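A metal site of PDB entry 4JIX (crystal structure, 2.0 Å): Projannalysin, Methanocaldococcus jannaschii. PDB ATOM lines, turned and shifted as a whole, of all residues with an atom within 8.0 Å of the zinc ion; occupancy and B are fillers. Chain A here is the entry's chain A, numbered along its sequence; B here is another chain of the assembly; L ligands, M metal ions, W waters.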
ATOM      1  N   ALA A  41     -22.564   9.829  13.140  1.00  0.00           N
ATOM      2  CA  ALA A  41     -23.585   9.713  12.093  1.00  0.00           C
ATOM      3  C   ALA A  41     -24.974   9.487  12.668  1.00  0.00           C
ATOM      4  O   ALA A  41     -25.132   8.874  13.724  1.00  0.00           O
ATOM      5  CB  ALA A  41     -23.238   8.598  11.117  1.00  0.00           C
ATOM      6  N   HIS A  71     -24.874   1.517   7.574  1.00  0.00           N
ATOM      7  CA  HIS A  71     -25.666   1.319   8.798  1.00  0.00           C
ATOM      8  C   HIS A  71     -26.916   2.222   8.796  1.00  0.00           C
ATOM      9  O   HIS A  71     -28.019   1.734   8.995  1.00  0.00           O
ATOM     10  CB  HIS A  71     -24.810   1.604  10.067  1.00  0.00           C
ATOM     11  CG  HIS A  71     -25.571   1.335  11.343  1.00  0.00           C
ATOM     12  ND1 HIS A  71     -25.422   0.141  12.029  1.00  0.00           N
ATOM     13  CD2 HIS A  71     -26.474   2.101  11.986  1.00  0.00           C
ATOM     14  CE1 HIS A  71     -26.222   0.225  13.088  1.00  0.00           C
ATOM     15  NE2 HIS A  71     -26.907   1.385  13.090  1.00  0.00           N
ATOM     16  N   GLU A  72     -26.734   3.532   8.580  1.00  0.00           N
ATOM     17  CA  GLU A  72     -27.871   4.473   8.596  1.00  0.00           C
ATOM     18  C   GLU A  72     -28.902   4.193   7.518  1.00  0.00           C
ATOM     19  O   GLU A  72     -30.103   4.383   7.731  1.00  0.00           O
ATOM     20  CB  GLU A  72     -27.377   5.919   8.408  1.00  0.00           C
ATOM     21  CG  GLU A  72     -26.226   6.327   9.304  1.00  0.00           C
ATOM     22  CD  GLU A  72     -26.511   6.220  10.779  1.00  0.00           C
ATOM     23  OE1 GLU A  72     -27.698   6.190  11.173  1.00  0.00           O
ATOM     24  OE2 GLU A  72     -25.528   6.123  11.549  1.00  0.00           O
ATOM     25  N   HIS A  75     -31.329   1.208   8.074  1.00  0.00           N
ATOM     26  CA  HIS A  75     -32.461   1.660   8.902  1.00  0.00           C
ATOM     27  C   HIS A  75     -33.528   2.314   8.014  1.00  0.00           C
ATOM     28  O   HIS A  75     -34.711   2.017   8.154  1.00  0.00           O
ATOM     29  CB  HIS A  75     -32.002   2.679   9.962  1.00  0.00           C
ATOM     30  CG  HIS A  75     -31.306   2.090  11.144  1.00  0.00           C
ATOM     31  ND1 HIS A  75     -31.932   1.177  11.972  1.00  0.00           N
ATOM     32  CD2 HIS A  75     -30.064   2.338  11.621  1.00  0.00           C
ATOM     33  CE1 HIS A  75     -31.053   0.895  12.920  1.00  0.00           C
ATOM     34  NE2 HIS A  75     -29.919   1.572  12.744  1.00  0.00           N
ATOM     35  N   SER A  80     -37.068   1.074  10.153  1.00  0.00           N
ATOM     36  CA  SER A  80     -36.948   0.707  11.558  1.00  0.00           C
ATOM     37  C   SER A  80     -35.714   1.325  12.149  1.00  0.00           C
ATOM     38  O   SER A  80     -34.651   1.252  11.535  1.00  0.00           O
ATOM     39  CB  SER A  80     -36.885  -0.815  11.722  1.00  0.00           C
ATOM     40  OG  SER A  80     -36.733  -1.172  13.092  1.00  0.00           O
ATOM     41  N   ILE A  81     -35.842   1.907  13.357  1.00  0.00           N
ATOM     42  CA  ILE A  81     -34.699   2.462  14.088  1.00  0.00           C
ATOM     43  C   ILE A  81     -33.973   1.334  14.856  1.00  0.00           C
ATOM     44  O   ILE A  81     -32.927   1.581  15.460  1.00  0.00           O
ATOM     45  CB  ILE A  81     -35.126   3.611  15.036  1.00  0.00           C
ATOM     46  CG1 ILE A  81     -36.047   3.095  16.168  1.00  0.00           C
ATOM     47  CG2 ILE A  81     -35.757   4.782  14.231  1.00  0.00           C
ATOM     48  CD1 ILE A  81     -36.171   4.022  17.392  1.00  0.00           C
ATOM     49  N   ASN A  82     -34.517   0.109  14.835  1.00  0.00           N
ATOM     50  CA  ASN A  82     -33.967  -1.027  15.571  1.00  0.00           C
ATOM     51  C   ASN A  82     -33.003  -1.878  14.721  1.00  0.00           C
ATOM     52  O   ASN A  82     -32.885  -1.685  13.505  1.00  0.00           O
ATOM     53  CB  ASN A  82     -35.108  -1.905  16.108  1.00  0.00           C
ATOM     54  CG  ASN A  82     -36.024  -1.182  17.058  1.00  0.00           C
ATOM     55  OD1 ASN A  82     -35.618  -0.258  17.769  1.00  0.00           O
ATOM     56  ND2 ASN A  82     -37.290  -1.570  17.107  1.00  0.00           N
ATOM     57  N   HIS A  83     -32.270  -2.769  15.391  1.00  0.00           N
ATOM     58  CA  HIS A  83     -31.307  -3.668  14.780  1.00  0.00           C
ATOM     59  C   HIS A  83     -31.822  -5.108  14.923  1.00  0.00           C
ATOM     60  O   HIS A  83     -31.150  -5.971  15.467  1.00  0.00           O
ATOM     61  CB  HIS A  83     -29.903  -3.498  15.394  1.00  0.00           C
ATOM     62  CG  HIS A  83     -29.450  -2.066  15.484  1.00  0.00           C
ATOM     63  ND1 HIS A  83     -29.325  -1.445  16.706  1.00  0.00           N
ATOM     64  CD2 HIS A  83     -29.108  -1.204  14.516  1.00  0.00           C
ATOM     65  CE1 HIS A  83     -28.941  -0.208  16.441  1.00  0.00           C
ATOM     66  NE2 HIS A  83     -28.792  -0.014  15.129  1.00  0.00           N
ATOM     67  N   PHE A  87     -32.760  -5.994  10.104  1.00  0.00           N
ATOM     68  CA  PHE A  87     -31.551  -5.183   9.962  1.00  0.00           C
ATOM     69  C   PHE A  87     -30.389  -6.106   9.592  1.00  0.00           C
ATOM     70  O   PHE A  87     -29.680  -5.837   8.613  1.00  0.00           O
ATOM     71  CB  PHE A  87     -31.233  -4.400  11.258  1.00  0.00           C
ATOM     72  CG  PHE A  87     -30.127  -3.390  11.082  1.00  0.00           C
ATOM     73  CD1 PHE A  87     -30.409  -2.055  10.830  1.00  0.00           C
ATOM     74  CD2 PHE A  87     -28.788  -3.785  11.135  1.00  0.00           C
ATOM     75  CE1 PHE A  87     -29.385  -1.125  10.625  1.00  0.00           C
ATOM     76  CE2 PHE A  87     -27.759  -2.858  10.900  1.00  0.00           C
ATOM     77  CZ  PHE A  87     -28.067  -1.536  10.654  1.00  0.00           C
ATOM     78  N   ILE B 108     -20.371   1.467  19.524  1.00  0.00           N
ATOM     79  CA  ILE B 108     -20.748   1.724  18.120  1.00  0.00           C
ATOM     80  C   ILE B 108     -22.196   2.214  18.010  1.00  0.00           C
ATOM     81  O   ILE B 108     -22.472   3.152  17.258  1.00  0.00           O
ATOM     82  CB  ILE B 108     -20.519   0.437  17.258  1.00  0.00           C
ATOM     83  CG1 ILE B 108     -19.019   0.208  17.033  1.00  0.00           C
ATOM     84  CG2 ILE B 108     -21.271   0.506  15.901  1.00  0.00           C
ATOM     85  CD1 ILE B 108     -18.265   1.279  16.074  1.00  0.00           C
ATOM     86  N   GLN B 109     -23.109   1.627  18.792  1.00  0.00           N
ATOM     87  CA  GLN B 109     -24.519   1.971  18.750  1.00  0.00           C
ATOM     88  C   GLN B 109     -24.775   3.366  19.385  1.00  0.00           C
ATOM     89  O   GLN B 109     -25.777   3.989  19.062  1.00  0.00           O
ATOM     90  CB  GLN B 109     -25.364   0.858  19.369  1.00  0.00           C
ATOM     91  CG  GLN B 109     -25.374  -0.398  18.471  1.00  0.00           C
ATOM     92  CD  GLN B 109     -26.135  -1.578  19.049  1.00  0.00           C
ATOM     93  OE1 GLN B 109     -26.400  -1.665  20.251  1.00  0.00           O
ATOM     94  NE2 GLN B 109     -26.444  -2.555  18.197  1.00  0.00           N
ATOM     95  N   LYS B 110     -23.825   3.885  20.176  1.00  0.00           N
ATOM     96  CA  LYS B 110     -23.838   5.248  20.725  1.00  0.00           C
ATOM     97  C   LYS B 110     -23.308   6.249  19.669  1.00  0.00           C
ATOM     98  O   LYS B 110     -23.654   7.432  19.712  1.00  0.00           O
ATOM     99  CB  LYS B 110     -22.980   5.302  22.002  1.00  0.00           C
ATOM    100  CG  LYS B 110     -23.640   6.003  23.174  1.00  0.00           C
ATOM    101  CD  LYS B 110     -24.604   5.139  23.956  1.00  0.00           C
ATOM    102  CE  LYS B 110     -25.094   5.874  25.178  1.00  0.00           C
ATOM    103  NZ  LYS B 110     -26.009   6.993  24.845  1.00  0.00           N
ATOM    104  N   LEU B 111     -22.462   5.788  18.717  1.00  0.00           N
ATOM    105  CA  LEU B 111     -21.843   6.658  17.707  1.00  0.00           C
ATOM    106  C   LEU B 111     -22.598   6.750  16.399  1.00  0.00           C
ATOM    107  O   LEU B 111     -22.554   7.802  15.758  1.00  0.00           O
ATOM    108  CB  LEU B 111     -20.413   6.177  17.406  1.00  0.00           C
ATOM    109  CG  LEU B 111     -19.406   6.216  18.558  1.00  0.00           C
ATOM    110  CD1 LEU B 111     -18.153   5.463  18.203  1.00  0.00           C
ATOM    111  CD2 LEU B 111     -19.124   7.632  18.995  1.00  0.00           C
ATOM    112  N   ILE B 112     -23.219   5.645  15.947  1.00  0.00           N
ATOM    113  CA  ILE B 112     -23.922   5.606  14.657  1.00  0.00           C
ATOM    114  C   ILE B 112     -25.344   5.058  14.822  1.00  0.00           C
ATOM    115  O   ILE B 112     -26.162   5.280  13.900  1.00  0.00           O
ATOM    116  CB  ILE B 112     -23.093   4.803  13.606  1.00  0.00           C
ATOM    117  CG1 ILE B 112     -23.080   3.278  13.904  1.00  0.00           C
ATOM    118  CG2 ILE B 112     -21.658   5.347  13.474  1.00  0.00           C
ATOM    119  CD1 ILE B 112     -22.375   2.387  12.805  1.00  0.00           C
ATOM    120  OXT ILE B 112     -25.634   4.422  15.866  1.00  0.00           O
HETATM  121  C1  LIG L   1     -30.057   4.283  15.384  1.00  0.00           C
HETATM  122  C2  LIG L   1     -29.381   4.956  16.591  1.00  0.00           C
HETATM  123  C3  LIG L   1     -31.531   4.676  15.256  1.00  0.00           C
HETATM  124  C4  LIG L   1     -29.314   4.631  14.099  1.00  0.00           C
HETATM  125  N1  LIG L   1     -29.985   2.791  15.599  1.00  0.00           N
HETATM  126  O1  LIG L   1     -29.978   4.563  17.825  1.00  0.00           O
HETATM  127  O2  LIG L   1     -31.669   6.039  14.865  1.00  0.00           O
HETATM  128  O3  LIG L   1     -28.252   3.729  13.831  1.00  0.00           O
HETATM  129 ZN    ZN M   1     -28.517   1.874  14.327  1.00  0.00          ZN
HETATM  130  O   HOH W   1     -27.121   2.231  15.966  1.00  0.00           O
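ND1 of His 75 is in hydrogen-bond range of O of Ser 80. A ring nitrogen (ND1) of His 83 lies within hydrogen-bond range of the side-chain amide nitrogen (NE2) of Gln 109 of chain B, at 3.4 Å. The backbone carbonyl oxygen of Asn 82 sits close to a ring nitrogen (ND1) of His 75, 3.4 Å away.
The zinc ion is bound by an oxygen (O3) of the ligand (1.9 Å), a ring nitrogen (NE2) of His 83 (2.1 Å), a ring nitrogen (NE2) of His 71 (2.1 Å), a ring nitrogen (NE2) of His 75 (2.1 Å), a nitrogen (N1) of the ligand (2.1 Å) and water W1 (2.2 Å).
Within 4 Å of the zinc ion: His 71, His 75 and His 83. The nearest printed residue that does not touch the zinc ion is Ile 112 of chain B (4.1 Å).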
